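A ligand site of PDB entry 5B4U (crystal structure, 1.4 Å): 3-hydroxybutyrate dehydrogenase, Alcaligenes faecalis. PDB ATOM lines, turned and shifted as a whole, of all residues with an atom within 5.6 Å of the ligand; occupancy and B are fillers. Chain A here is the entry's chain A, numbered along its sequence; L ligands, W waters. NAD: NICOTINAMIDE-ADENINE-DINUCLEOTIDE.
Water W3 lies within hydrogen-bond range of O2B of the ligand (2.7 Å) and O of Phe 36 (3.3 Å).
Water W5 lies within hydrogen-bond range of the backbone carbonyl oxygen of Gly 92 and an oxygen (O1A) of the ligand.
The backbone carbonyl oxygen (O) of Gly 186 lies close to an oxygen (O7N) of the ligand.
Ser 12 touches the ligand.
Gly 15 touches the ligand (CA to O2N, 3.5 Å).
Asn 34 touches the ligand (OD1 to C2A, 3.7 Å).
Gly 35 touches the ligand (CA to N3A, 3.7 Å).
Ala 62 touches the ligand (O to C2A, 3.4 Å).
Ala 91 touches the ligand.
Gly 92 touches the ligand.
CG2 of Ile 93 touches N7A of the ligand, 3.99 Å away.
Leu 113 touches the ligand.
CG2 of Ile 140 touches O4D of the ligand, 3.5 Å away.
O of Ala 141 touches C6N of the ligand, 3.1 Å away.
Ser 142 touches the ligand (OG to C5N, 3.7 Å).
Pro 185 touches the ligand (O to C5N, 3.4 Å).
Trp 187 touches the ligand.
Pro 191 touches the ligand.
Leu 192 touches the ligand.
Val 193 touches the ligand.
Hydrophobic or aromatic side chains that line the ligand: Ile 16, Phe 36, Leu 64, Ala 91, Ile 93, Leu 113, Ile 140, Tyr 155, Pro 185, Val 188, Pro 191, Leu 192 and Val 193.
N of Asn 90 is in hydrogen-bond range of OG1 of Thr 10, at 2.8 Å.
The backbone NH (N) of Thr 13 is in hydrogen-bond range of the backbone carbonyl oxygen (O) of Asn 34, at 3.4 Å.
The backbone NH of Gly 11 is in hydrogen-bond range of the side-chain amide oxygen of Asn 34 (3.0 Å).
The backbone NH (N) of Ala 143 lies within hydrogen-bond range of the backbone carbonyl oxygen (O) of Pro 185.
The backbone carbonyl oxygen of Ala 62 sits at hydrogen-bond distance from the side-chain amide nitrogen of Asn 34 (3.3 Å).
The backbone carbonyl oxygen of Asn 34 is in hydrogen-bond range of the backbone NH of Ser 12 (2.7 Å).
O of Ser 142 lies close to SG of Cys 184.
The backbone NH (N) of Ala 91 lies within hydrogen-bond range of the side-chain hydroxyl (OG1) of Thr 10 (3.0 Å).
O1N of the ligand lies within hydrogen-bond range of OG1 of Thr 190, 2.6 Å away.
OH of Tyr 155 is in hydrogen-bond range of O2D of the ligand (2.7 Å).
The backbone carbonyl oxygen (O) of Asn 90 is in hydrogen-bond range of an oxygen (O3D) of the ligand (2.7 Å).
O7N of the ligand lies within hydrogen-bond range of N of Val 188 (2.8 Å).
N7N of the ligand is in hydrogen-bond range of O of Val 188.
The backbone NH (N) of Thr 13 is in hydrogen-bond range of an oxygen (O3B) of the ligand.
OG1 of Thr 13 is in hydrogen-bond range of O3B of the ligand.
The backbone NH of Ser 14 lies within hydrogen-bond range of an oxygen (O3B) of the ligand (3.4 Å).
The side-chain hydroxyl (OG) of Ser 14 lies within hydrogen-bond range of an oxygen (O2A) of the ligand, 2.8 Å away.
An oxygen (O2N) of the ligand is in hydrogen-bond range of the backbone NH (N) of Ile 16.
An oxygen (O2B) of the ligand lies within hydrogen-bond range of the backbone NH (N) of Phe 36, at 2.9 Å.
O2B of the ligand sits at hydrogen-bond distance from O of Phe 36 (3.5 Å).
A nitrogen (N6A) of the ligand is in hydrogen-bond range of the side-chain carboxylate (OD1) of Asp 63 (2.9 Å).
The side-chain amino group of Lys 159 lies within hydrogen-bond range of an oxygen (O3D) of the ligand, at 2.9 Å.
N of Leu 64 lies within hydrogen-bond range of N1A of the ligand, 3.0 Å away.
The backbone carbonyl oxygen (O) of Gly 11 sits at hydrogen-bond distance from an oxygen (O3B) of the ligand, 3.2 Å away.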
ATOM      1  N   THR A  10      -9.472  -1.348  16.017  1.00  0.00           N
ATOM      2  CA  THR A  10      -9.469  -2.724  15.556  1.00  0.00           C
ATOM      3  C   THR A  10      -9.397  -2.763  14.040  1.00  0.00           C
ATOM      4  O   THR A  10      -9.830  -1.821  13.359  1.00  0.00           O
ATOM      5  CB  THR A  10     -10.711  -3.498  16.043  1.00  0.00           C
ATOM      6  OG1 THR A  10     -11.875  -3.021  15.364  1.00  0.00           O
ATOM      7  CG2 THR A  10     -10.904  -3.353  17.539  1.00  0.00           C
ATOM      8  N   GLY A  11      -8.787  -3.809  13.495  1.00  0.00           N
ATOM      9  CA  GLY A  11      -8.660  -3.936  12.052  1.00  0.00           C
ATOM     10  C   GLY A  11      -7.972  -2.725  11.447  1.00  0.00           C
ATOM     11  O   GLY A  11      -8.429  -2.188  10.439  1.00  0.00           O
ATOM     12  N   SER A  12      -6.810  -2.370  11.993  1.00  0.00           N
ATOM     13  CA  SER A  12      -6.105  -1.172  11.580  1.00  0.00           C
ATOM     14  C   SER A  12      -4.781  -1.492  10.886  1.00  0.00           C
ATOM     15  O   SER A  12      -3.957  -0.610  10.686  1.00  0.00           O
ATOM     16  CB  SER A  12      -5.858  -0.253  12.780  1.00  0.00           C
ATOM     17  OG  SER A  12      -5.408  -0.989  13.911  1.00  0.00           O
ATOM     18  N   THR A  13      -4.696  -2.688  10.311  1.00  0.00           N
ATOM     19  CA  THR A  13      -3.532  -3.068   9.498  1.00  0.00           C
ATOM     20  C   THR A  13      -3.778  -2.853   8.008  1.00  0.00           C
ATOM     21  O   THR A  13      -2.903  -3.107   7.177  1.00  0.00           O
ATOM     22  CB  THR A  13      -3.165  -4.547   9.722  1.00  0.00           C
ATOM     23  OG1 THR A  13      -4.318  -5.377   9.507  1.00  0.00           O
ATOM     24  CG2 THR A  13      -2.656  -4.756  11.138  1.00  0.00           C
ATOM     25  N   SER A  14      -4.956  -2.348   7.669  1.00  0.00           N
ATOM     26  CA  SER A  14      -5.358  -2.147   6.275  1.00  0.00           C
ATOM     27  C   SER A  14      -6.423  -1.070   6.243  1.00  0.00           C
ATOM     28  O   SER A  14      -7.135  -0.860   7.228  1.00  0.00           O
ATOM     29  CB  SER A  14      -5.918  -3.444   5.683  1.00  0.00           C
ATOM     30  OG  SER A  14      -6.401  -3.263   4.360  1.00  0.00           O
ATOM     31  N   GLY A  15      -6.598  -0.463   5.074  1.00  0.00           N
ATOM     32  CA  GLY A  15      -7.845   0.220   4.745  1.00  0.00           C
ATOM     33  C   GLY A  15      -8.178   1.314   5.739  1.00  0.00           C
ATOM     34  O   GLY A  15      -7.350   2.147   6.083  1.00  0.00           O
ATOM     35  N   ILE A  16      -9.470   1.413   6.043  1.00  0.00           N
ATOM     36  CA  ILE A  16      -9.989   2.508   6.818  1.00  0.00           C
ATOM     37  C   ILE A  16      -9.344   2.578   8.199  1.00  0.00           C
ATOM     38  O   ILE A  16      -8.993   3.652   8.679  1.00  0.00           O
ATOM     39  CB  ILE A  16     -11.522   2.371   6.945  1.00  0.00           C
ATOM     40  CG1 ILE A  16     -12.176   2.578   5.573  1.00  0.00           C
ATOM     41  CG2 ILE A  16     -12.076   3.339   7.971  1.00  0.00           C
ATOM     42  CD1 ILE A  16     -13.613   2.124   5.499  1.00  0.00           C
ATOM     43  N   GLY A  17      -9.166   1.420   8.828  1.00  0.00           N
ATOM     44  CA  GLY A  17      -8.610   1.353  10.173  1.00  0.00           C
ATOM     45  C   GLY A  17      -7.191   1.880  10.251  1.00  0.00           C
ATOM     46  O   GLY A  17      -6.810   2.545  11.205  1.00  0.00           O
ATOM     47  N   ASN A  34      -4.169  -3.423  15.289  1.00  0.00           N
ATOM     48  CA  ASN A  34      -4.718  -4.766  15.390  1.00  0.00           C
ATOM     49  C   ASN A  34      -5.107  -5.201  13.993  1.00  0.00           C
ATOM     50  O   ASN A  34      -5.415  -4.362  13.149  1.00  0.00           O
ATOM     51  CB  ASN A  34      -5.948  -4.756  16.320  1.00  0.00           C
ATOM     52  CG  ASN A  34      -6.836  -5.960  16.114  1.00  0.00           C
ATOM     53  OD1 ASN A  34      -7.857  -5.880  15.425  1.00  0.00           O
ATOM     54  ND2 ASN A  34      -6.522  -7.055  16.798  1.00  0.00           N
ATOM     55  N   GLY A  35      -5.047  -6.500  13.727  1.00  0.00           N
ATOM     56  CA  GLY A  35      -5.498  -7.033  12.450  1.00  0.00           C
ATOM     57  C   GLY A  35      -4.491  -7.998  11.854  1.00  0.00           C
ATOM     58  O   GLY A  35      -3.405  -8.195  12.396  1.00  0.00           O
ATOM     59  N   PHE A  36      -4.827  -8.520  10.686  1.00  0.00           N
ATOM     60  CA  PHE A  36      -4.003  -9.505  10.024  1.00  0.00           C
ATOM     61  C   PHE A  36      -3.119  -8.827   8.993  1.00  0.00           C
ATOM     62  O   PHE A  36      -3.334  -7.678   8.622  1.00  0.00           O
ATOM     63  CB  PHE A  36      -4.877 -10.574   9.368  1.00  0.00           C
ATOM     64  CG  PHE A  36      -5.793 -11.279  10.328  1.00  0.00           C
ATOM     65  CD1 PHE A  36      -5.378 -11.562  11.622  1.00  0.00           C
ATOM     66  CD2 PHE A  36      -7.127 -11.491  10.001  1.00  0.00           C
ATOM     67  CE1 PHE A  36      -6.241 -12.180  12.513  1.00  0.00           C
ATOM     68  CE2 PHE A  36      -7.946 -12.205  10.847  1.00  0.00           C
ATOM     69  CZ  PHE A  36      -7.503 -12.556  12.101  1.00  0.00           C
ATOM     70  N   GLY A  37      -2.095  -9.542   8.535  1.00  0.00           N
ATOM     71  CA  GLY A  37      -1.228  -9.030   7.485  1.00  0.00           C
ATOM     72  C   GLY A  37       0.171  -9.604   7.612  1.00  0.00           C
ATOM     73  O   GLY A  37       0.440 -10.381   8.532  1.00  0.00           O
ATOM     74  N   ALA A  62      -5.104 -10.144  17.576  1.00  0.00           N
ATOM     75  CA  ALA A  62      -6.250 -10.833  18.139  1.00  0.00           C
ATOM     76  C   ALA A  62      -7.268 -11.052  17.043  1.00  0.00           C
ATOM     77  O   ALA A  62      -7.522 -10.148  16.246  1.00  0.00           O
ATOM     78  CB  ALA A  62      -6.863 -10.007  19.256  1.00  0.00           C
ATOM     79  N   ASP A  63      -7.715 -12.289  16.908  1.00  0.00           N
ATOM     80  CA  ASP A  63      -8.831 -12.610  16.019  1.00  0.00           C
ATOM     81  C   ASP A  63     -10.142 -12.303  16.726  1.00  0.00           C
ATOM     82  O   ASP A  63     -10.519 -12.976  17.689  1.00  0.00           O
ATOM     83  CB  ASP A  63      -8.773 -14.089  15.629  1.00  0.00           C
ATOM     84  CG  ASP A  63      -9.880 -14.477  14.658  1.00  0.00           C
ATOM     85  OD1 ASP A  63     -10.887 -13.755  14.586  1.00  0.00           O
ATOM     86  OD2 ASP A  63      -9.808 -15.600  14.112  1.00  0.00           O
ATOM     87  N   LEU A  64     -10.753 -11.192  16.355  1.00  0.00           N
ATOM     88  CA  LEU A  64     -11.867 -10.639  17.115  1.00  0.00           C
ATOM     89  C   LEU A  64     -13.195 -11.333  16.800  1.00  0.00           C
ATOM     90  O   LEU A  64     -14.219 -10.976  17.381  1.00  0.00           O
ATOM     91  CB  LEU A  64     -11.999  -9.145  16.853  1.00  0.00           C
ATOM     92  CG  LEU A  64     -10.730  -8.344  17.162  1.00  0.00           C
ATOM     93  CD1 LEU A  64     -10.935  -6.882  16.805  1.00  0.00           C
ATOM     94  CD2 LEU A  64     -10.347  -8.487  18.623  1.00  0.00           C
ATOM     95  N   SER A  65     -13.142 -12.418  16.035  1.00  0.00           N
ATOM     96  CA  SER A  65     -14.318 -13.267  15.869  1.00  0.00           C
ATOM     97  C   SER A  65     -14.564 -14.118  17.097  1.00  0.00           C
ATOM     98  O   SER A  65     -15.608 -14.748  17.232  1.00  0.00           O
ATOM     99  CB  SER A  65     -14.171 -14.147  14.632  1.00  0.00           C
ATOM    100  OG  SER A  65     -13.170 -15.126  14.823  1.00  0.00           O
ATOM    101  N   ASN A  90     -13.662  -1.225  14.222  1.00  0.00           N
ATOM    102  CA  ASN A  90     -13.583  -1.050  12.780  1.00  0.00           C
ATOM    103  C   ASN A  90     -13.465  -2.363  11.998  1.00  0.00           C
ATOM    104  O   ASN A  90     -13.930  -2.461  10.870  1.00  0.00           O
ATOM    105  CB  ASN A  90     -12.424  -0.124  12.431  1.00  0.00           C
ATOM    106  CG  ASN A  90     -12.038  -0.183  10.970  1.00  0.00           C
ATOM    107  OD1 ASN A  90     -12.637   0.485  10.131  1.00  0.00           O
ATOM    108  ND2 ASN A  90     -11.042  -0.994  10.662  1.00  0.00           N
ATOM    109  N   ALA A  91     -12.833  -3.383  12.589  1.00  0.00           N
ATOM    110  CA  ALA A  91     -12.571  -4.617  11.860  1.00  0.00           C
ATOM    111  C   ALA A  91     -13.858  -5.170  11.257  1.00  0.00           C
ATOM    112  O   ALA A  91     -14.886  -5.221  11.916  1.00  0.00           O
ATOM    113  CB  ALA A  91     -11.937  -5.650  12.780  1.00  0.00           C
ATOM    114  N   GLY A  92     -13.794  -5.620  10.003  1.00  0.00           N
ATOM    115  CA  GLY A  92     -14.973  -6.164   9.361  1.00  0.00           C
ATOM    116  C   GLY A  92     -14.617  -6.932   8.107  1.00  0.00           C
ATOM    117  O   GLY A  92     -13.560  -6.703   7.520  1.00  0.00           O
ATOM    118  N   ILE A  93     -15.507  -7.845   7.716  1.00  0.00           N
ATOM    119  CA  ILE A  93     -15.363  -8.588   6.476  1.00  0.00           C
ATOM    120  C   ILE A  93     -16.655  -8.545   5.663  1.00  0.00           C
ATOM    121  O   ILE A  93     -17.712  -8.135   6.166  1.00  0.00           O
ATOM    122  CB  ILE A  93     -14.966 -10.061   6.744  1.00  0.00           C
ATOM    123  CG1 ILE A  93     -15.947 -10.699   7.727  1.00  0.00           C
ATOM    124  CG2 ILE A  93     -13.551 -10.140   7.278  1.00  0.00           C
ATOM    125  CD1 ILE A  93     -15.763 -12.192   7.869  1.00  0.00           C
ATOM    126  N   LEU A 113     -17.702 -11.110  13.636  1.00  0.00           N
ATOM    127  CA  LEU A 113     -16.743 -10.012  13.568  1.00  0.00           C
ATOM    128  C   LEU A 113     -17.440  -8.658  13.486  1.00  0.00           C
ATOM    129  O   LEU A 113     -17.103  -7.734  14.220  1.00  0.00           O
ATOM    130  CB  LEU A 113     -15.798 -10.187  12.392  1.00  0.00           C
ATOM    131  CG  LEU A 113     -14.716  -9.113  12.308  1.00  0.00           C
ATOM    132  CD1 LEU A 113     -13.835  -9.117  13.548  1.00  0.00           C
ATOM    133  CD2 LEU A 113     -13.898  -9.299  11.042  1.00  0.00           C
ATOM    134  N   ASN A 114     -18.367  -8.540  12.540  1.00  0.00           N
ATOM    135  CA  ASN A 114     -18.935  -7.242  12.213  1.00  0.00           C
ATOM    136  C   ASN A 114     -19.937  -6.753  13.259  1.00  0.00           C
ATOM    137  O   ASN A 114     -20.237  -5.561  13.310  1.00  0.00           O
ATOM    138  CB  ASN A 114     -19.617  -7.280  10.848  1.00  0.00           C
ATOM    139  CG  ASN A 114     -18.647  -7.447   9.693  1.00  0.00           C
ATOM    140  OD1 ASN A 114     -17.567  -8.002   9.844  1.00  0.00           O
ATOM    141  ND2 ASN A 114     -19.060  -7.011   8.513  1.00  0.00           N
ATOM    142  N   ILE A 140     -17.608   1.643  13.288  1.00  0.00           N
ATOM    143  CA  ILE A 140     -17.639   1.810  11.849  1.00  0.00           C
ATOM    144  C   ILE A 140     -18.693   0.893  11.268  1.00  0.00           C
ATOM    145  O   ILE A 140     -18.538  -0.326  11.250  1.00  0.00           O
ATOM    146  CB  ILE A 140     -16.276   1.498  11.193  1.00  0.00           C
ATOM    147  CG1 ILE A 140     -15.157   2.263  11.893  1.00  0.00           C
ATOM    148  CG2 ILE A 140     -16.325   1.826   9.706  1.00  0.00           C
ATOM    149  CD1 ILE A 140     -15.361   3.762  11.952  1.00  0.00           C
ATOM    150  N   ALA A 141     -19.861   1.475  11.007  1.00  0.00           N
ATOM    151  CA  ALA A 141     -20.952   0.738  10.391  1.00  0.00           C
ATOM    152  C   ALA A 141     -20.830   0.856   8.882  1.00  0.00           C
ATOM    153  O   ALA A 141     -19.801   0.484   8.320  1.00  0.00           O
ATOM    154  CB  ALA A 141     -22.289   1.237  10.895  1.00  0.00           C
ATOM    155  N   SER A 142     -21.815   1.470   8.241  1.00  0.00           N
ATOM    156  CA  SER A 142     -21.902   1.508   6.780  1.00  0.00           C
ATOM    157  C   SER A 142     -23.203   2.211   6.419  1.00  0.00           C
ATOM    158  O   SER A 142     -24.124   2.234   7.219  1.00  0.00           O
ATOM    159  CB  SER A 142     -21.902   0.097   6.214  1.00  0.00           C
ATOM    160  OG  SER A 142     -22.096   0.107   4.804  1.00  0.00           O
ATOM    161  N   ALA A 143     -23.313   2.692   5.185  1.00  0.00           N
ATOM    162  CA  ALA A 143     -24.627   2.978   4.627  1.00  0.00           C
ATOM    163  C   ALA A 143     -25.526   1.747   4.728  1.00  0.00           C
ATOM    164  O   ALA A 143     -26.747   1.875   4.897  1.00  0.00           O
ATOM    165  CB  ALA A 143     -24.513   3.440   3.188  1.00  0.00           C
ATOM    166  N   TYR A 155     -24.056  -9.004   6.029  1.00  0.00           N
ATOM    167  CA  TYR A 155     -23.378  -7.732   6.234  1.00  0.00           C
ATOM    168  C   TYR A 155     -24.369  -6.623   6.594  1.00  0.00           C
ATOM    169  O   TYR A 155     -24.162  -5.883   7.548  1.00  0.00           O
ATOM    170  CB  TYR A 155     -22.612  -7.373   4.969  1.00  0.00           C
ATOM    171  CG  TYR A 155     -21.744  -6.142   5.105  1.00  0.00           C
ATOM    172  CD1 TYR A 155     -20.424  -6.244   5.499  1.00  0.00           C
ATOM    173  CD2 TYR A 155     -22.201  -4.899   4.684  1.00  0.00           C
ATOM    174  CE1 TYR A 155     -19.577  -5.159   5.462  1.00  0.00           C
ATOM    175  CE2 TYR A 155     -21.376  -3.794   4.712  1.00  0.00           C
ATOM    176  CZ  TYR A 155     -20.058  -3.935   5.053  1.00  0.00           C
ATOM    177  OH  TYR A 155     -19.219  -2.853   5.022  1.00  0.00           O
ATOM    178  N   LYS A 159     -24.511  -4.730  10.145  1.00  0.00           N
ATOM    179  CA  LYS A 159     -24.300  -3.299  10.206  1.00  0.00           C
ATOM    180  C   LYS A 159     -25.520  -2.571  10.766  1.00  0.00           C
ATOM    181  O   LYS A 159     -25.374  -1.626  11.542  1.00  0.00           O
ATOM    182  CB  LYS A 159     -23.927  -2.732   8.832  1.00  0.00           C
ATOM    183  CG  LYS A 159     -22.580  -3.199   8.303  1.00  0.00           C
ATOM    184  CD  LYS A 159     -21.437  -2.768   9.201  1.00  0.00           C
ATOM    185  CE  LYS A 159     -20.082  -2.961   8.530  1.00  0.00           C
ATOM    186  NZ  LYS A 159     -18.968  -2.528   9.405  1.00  0.00           N
ATOM    187  N   CYS A 184     -20.866   5.915   9.179  1.00  0.00           N
ATOM    188  CA  CYS A 184     -21.521   5.101   8.158  1.00  0.00           C
ATOM    189  C   CYS A 184     -21.002   5.496   6.778  1.00  0.00           C
ATOM    190  O   CYS A 184     -21.605   6.329   6.102  1.00  0.00           O
ATOM    191  CB  CYS A 184     -23.034   5.282   8.226  1.00  0.00           C
ATOM    192  SG  CYS A 184     -23.779   4.612   9.729  1.00  0.00           S
ATOM    193  N   PRO A 185     -19.864   4.927   6.376  1.00  0.00           N
ATOM    194  CA  PRO A 185     -19.316   5.278   5.070  1.00  0.00           C
ATOM    195  C   PRO A 185     -20.107   4.670   3.925  1.00  0.00           C
ATOM    196  O   PRO A 185     -20.663   3.578   4.061  1.00  0.00           O
ATOM    197  CB  PRO A 185     -17.897   4.695   5.101  1.00  0.00           C
ATOM    198  CG  PRO A 185     -17.637   4.289   6.516  1.00  0.00           C
ATOM    199  CD  PRO A 185     -18.991   4.004   7.109  1.00  0.00           C
ATOM    200  N   GLY A 186     -20.146   5.373   2.804  1.00  0.00           N
ATOM    201  CA  GLY A 186     -20.364   4.752   1.500  1.00  0.00           C
ATOM    202  C   GLY A 186     -19.101   4.064   0.996  1.00  0.00           C
ATOM    203  O   GLY A 186     -18.244   3.664   1.788  1.00  0.00           O
ATOM    204  N   TRP A 187     -19.005   3.879  -0.318  1.00  0.00           N
ATOM    205  CA  TRP A 187     -17.883   3.155  -0.890  1.00  0.00           C
ATOM    206  C   TRP A 187     -16.571   3.858  -0.559  1.00  0.00           C
ATOM    207  O   TRP A 187     -16.399   5.035  -0.841  1.00  0.00           O
ATOM    208  CB  TRP A 187     -18.003   3.052  -2.416  1.00  0.00           C
ATOM    209  CG  TRP A 187     -19.204   2.330  -2.915  1.00  0.00           C
ATOM    210  CD1 TRP A 187     -20.077   2.790  -3.863  1.00  0.00           C
ATOM    211  CD2 TRP A 187     -19.491   0.928  -2.757  1.00  0.00           C
ATOM    212  NE1 TRP A 187     -20.893   1.773  -4.297  1.00  0.00           N
ATOM    213  CE2 TRP A 187     -20.546   0.615  -3.645  1.00  0.00           C
ATOM    214  CE3 TRP A 187     -18.933  -0.099  -1.991  1.00  0.00           C
ATOM    215  CZ2 TRP A 187     -21.081  -0.661  -3.760  1.00  0.00           C
ATOM    216  CZ3 TRP A 187     -19.445  -1.381  -2.128  1.00  0.00           C
ATOM    217  CH2 TRP A 187     -20.509  -1.651  -3.012  1.00  0.00           C
ATOM    218  N   VAL A 188     -15.599   3.040  -0.138  1.00  0.00           N
ATOM    219  CA  VAL A 188     -14.213   3.441   0.073  1.00  0.00           C
ATOM    220  C   VAL A 188     -13.343   2.393  -0.604  1.00  0.00           C
ATOM    221  O   VAL A 188     -13.603   1.202  -0.483  1.00  0.00           O
ATOM    222  CB  VAL A 188     -13.883   3.437   1.584  1.00  0.00           C
ATOM    223  CG1 VAL A 188     -12.481   3.961   1.829  1.00  0.00           C
ATOM    224  CG2 VAL A 188     -14.915   4.235   2.359  1.00  0.00           C
ATOM    225  N   ARG A 189     -12.391   2.833  -1.426  1.00  0.00           N
ATOM    226  CA  ARG A 189     -11.678   1.896  -2.275  1.00  0.00           C
ATOM    227  C   ARG A 189     -10.559   1.186  -1.522  1.00  0.00           C
ATOM    228  O   ARG A 189      -9.379   1.527  -1.651  1.00  0.00           O
ATOM    229  CB  ARG A 189     -11.147   2.569  -3.530  1.00  0.00           C
ATOM    230  CG  ARG A 189     -10.753   1.558  -4.583  1.00  0.00           C
ATOM    231  CD  ARG A 189     -10.577   2.180  -5.944  1.00  0.00           C
ATOM    232  NE  ARG A 189     -10.405   1.147  -6.963  1.00  0.00           N
ATOM    233  CZ  ARG A 189     -10.300   1.381  -8.259  1.00  0.00           C
ATOM    234  NH1 ARG A 189     -10.321   2.628  -8.708  1.00  0.00           N
ATOM    235  NH2 ARG A 189      -9.993   0.386  -9.078  1.00  0.00           N
ATOM    236  N   THR A 190     -10.961   0.221  -0.707  1.00  0.00           N
ATOM    237  CA  THR A 190     -10.060  -0.651   0.031  1.00  0.00           C
ATOM    238  C   THR A 190     -10.094  -2.036  -0.622  1.00  0.00           C
ATOM    239  O   THR A 190     -10.921  -2.283  -1.485  1.00  0.00           O
ATOM    240  CB  THR A 190     -10.553  -0.804   1.472  1.00  0.00           C
ATOM    241  OG1 THR A 190     -11.782  -1.529   1.456  1.00  0.00           O
ATOM    242  CG2 THR A 190     -10.780   0.552   2.122  1.00  0.00           C
ATOM    243  N   PRO A 191      -9.339  -2.991  -0.062  1.00  0.00           N
ATOM    244  CA  PRO A 191      -9.373  -4.346  -0.618  1.00  0.00           C
ATOM    245  C   PRO A 191     -10.744  -4.999  -0.506  1.00  0.00           C
ATOM    246  O   PRO A 191     -11.140  -5.776  -1.384  1.00  0.00           O
ATOM    247  CB  PRO A 191      -8.351  -5.099   0.228  1.00  0.00           C
ATOM    248  CG  PRO A 191      -7.377  -4.052   0.647  1.00  0.00           C
ATOM    249  CD  PRO A 191      -8.156  -2.782   0.804  1.00  0.00           C
ATOM    250  N   LEU A 192     -11.531  -4.569   0.480  1.00  0.00           N
ATOM    251  CA  LEU A 192     -12.863  -5.115   0.688  1.00  0.00           C
ATOM    252  C   LEU A 192     -13.785  -4.751  -0.486  1.00  0.00           C
ATOM    253  O   LEU A 192     -14.642  -5.532  -0.884  1.00  0.00           O
ATOM    254  CB  LEU A 192     -13.437  -4.572   1.991  1.00  0.00           C
ATOM    255  CG  LEU A 192     -14.809  -5.088   2.435  1.00  0.00           C
ATOM    256  CD1 LEU A 192     -14.875  -5.149   3.956  1.00  0.00           C
ATOM    257  CD2 LEU A 192     -15.915  -4.195   1.876  1.00  0.00           C
ATOM    258  N   VAL A 193     -13.521  -3.589  -1.082  1.00  0.00           N
ATOM    259  CA  VAL A 193     -14.317  -3.112  -2.213  1.00  0.00           C
ATOM    260  C   VAL A 193     -13.662  -3.471  -3.543  1.00  0.00           C
ATOM    261  O   VAL A 193     -14.350  -3.741  -4.521  1.00  0.00           O
ATOM    262  CB  VAL A 193     -14.531  -1.593  -2.108  1.00  0.00           C
ATOM    263  CG1 VAL A 193     -14.945  -1.007  -3.440  1.00  0.00           C
ATOM    264  CG2 VAL A 193     -15.589  -1.301  -1.043  1.00  0.00           C
HETATM  265  PA  NAD L   1     -10.094  -3.967   4.822  1.00  0.00           P
HETATM  266  O1A NAD L   1     -10.302  -5.384   4.388  1.00  0.00           O
HETATM  267  O2A NAD L   1      -9.152  -3.052   4.084  1.00  0.00           O
HETATM  268  O5B NAD L   1      -9.622  -3.939   6.350  1.00  0.00           O
HETATM  269  C5B NAD L   1     -10.195  -4.851   7.280  1.00  0.00           C
HETATM  270  C4B NAD L   1      -9.314  -4.855   8.521  1.00  0.00           C
HETATM  271  O4B NAD L   1      -9.892  -5.751   9.470  1.00  0.00           O
HETATM  272  C3B NAD L   1      -7.911  -5.386   8.218  1.00  0.00           C
HETATM  273  O3B NAD L   1      -6.975  -4.722   9.081  1.00  0.00           O
HETATM  274  C2B NAD L   1      -8.033  -6.850   8.579  1.00  0.00           C
HETATM  275  O2B NAD L   1      -6.781  -7.486   8.864  1.00  0.00           O
HETATM  276  C1B NAD L   1      -8.913  -6.732   9.804  1.00  0.00           C
HETATM  277  N9A NAD L   1      -9.553  -8.004  10.172  1.00  0.00           N
HETATM  278  C8A NAD L   1     -10.243  -8.830   9.359  1.00  0.00           C
HETATM  279  N7A NAD L   1     -10.693  -9.906  10.047  1.00  0.00           N
HETATM  280  C5A NAD L   1     -10.324  -9.739  11.330  1.00  0.00           C
HETATM  281  C6A NAD L   1     -10.449 -10.508  12.583  1.00  0.00           C
HETATM  282  N6A NAD L   1     -11.115 -11.692  12.603  1.00  0.00           N
HETATM  283  N1A NAD L   1      -9.957  -9.944  13.703  1.00  0.00           N
HETATM  284  C2A NAD L   1      -9.249  -8.808  13.687  1.00  0.00           C
HETATM  285  N3A NAD L   1      -9.089  -8.056  12.580  1.00  0.00           N
HETATM  286  C4A NAD L   1      -9.648  -8.446  11.420  1.00  0.00           C
HETATM  287  O3  NAD L   1     -11.580  -3.347   4.871  1.00  0.00           O
HETATM  288  PN  NAD L   1     -12.092  -1.841   5.086  1.00  0.00           P
HETATM  289  O1N NAD L   1     -12.841  -1.483   3.833  1.00  0.00           O
HETATM  290  O2N NAD L   1     -11.004  -0.945   5.584  1.00  0.00           O
HETATM  291  O5D NAD L   1     -13.167  -2.099   6.245  1.00  0.00           O
HETATM  292  C5D NAD L   1     -13.037  -1.576   7.566  1.00  0.00           C
HETATM  293  C4D NAD L   1     -14.439  -1.365   8.110  1.00  0.00           C
HETATM  294  O4D NAD L   1     -15.108  -0.388   7.294  1.00  0.00           O
HETATM  295  C3D NAD L   1     -15.283  -2.631   8.046  1.00  0.00           C
HETATM  296  O3D NAD L   1     -16.094  -2.744   9.240  1.00  0.00           O
HETATM  297  C2D NAD L   1     -16.199  -2.393   6.867  1.00  0.00           C
HETATM  298  O2D NAD L   1     -17.433  -3.095   7.008  1.00  0.00           O
HETATM  299  C1D NAD L   1     -16.393  -0.891   6.958  1.00  0.00           C
HETATM  300  N1N NAD L   1     -16.885  -0.281   5.720  1.00  0.00           N
HETATM  301  C2N NAD L   1     -16.146  -0.310   4.598  1.00  0.00           C
HETATM  302  C3N NAD L   1     -16.607   0.347   3.457  1.00  0.00           C
HETATM  303  C7N NAD L   1     -15.862   0.301   2.162  1.00  0.00           C
HETATM  304  O7N NAD L   1     -16.418   0.760   1.178  1.00  0.00           O
HETATM  305  N7N NAD L   1     -14.623  -0.180   2.141  1.00  0.00           N
HETATM  306  C4N NAD L   1     -17.812   1.025   3.495  1.00  0.00           C
HETATM  307  C5N NAD L   1     -18.528   1.065   4.687  1.00  0.00           C
HETATM  308  C6N NAD L   1     -18.016   0.439   5.808  1.00  0.00           C
HETATM  309  O   HOH W   1     -12.751 -13.394  10.711  1.00  0.00           O
HETATM  310  O   HOH W   2      -9.963  -8.811   6.114  1.00  0.00           O
HETATM  311  O   HOH W   3      -5.842  -8.081   6.456  1.00  0.00           O
HETATM  312  O   HOH W   4     -11.026 -12.369   8.704  1.00  0.00           O
HETATM  313  O   HOH W   5     -12.115  -7.328   5.273  1.00  0.00           O
HETATM  314  O   HOH W   6      -7.860  -6.974   4.523  1.00  0.00           O
HETATM  315  O   HOH W   7      -9.834  -1.267   7.950  1.00  0.00           O
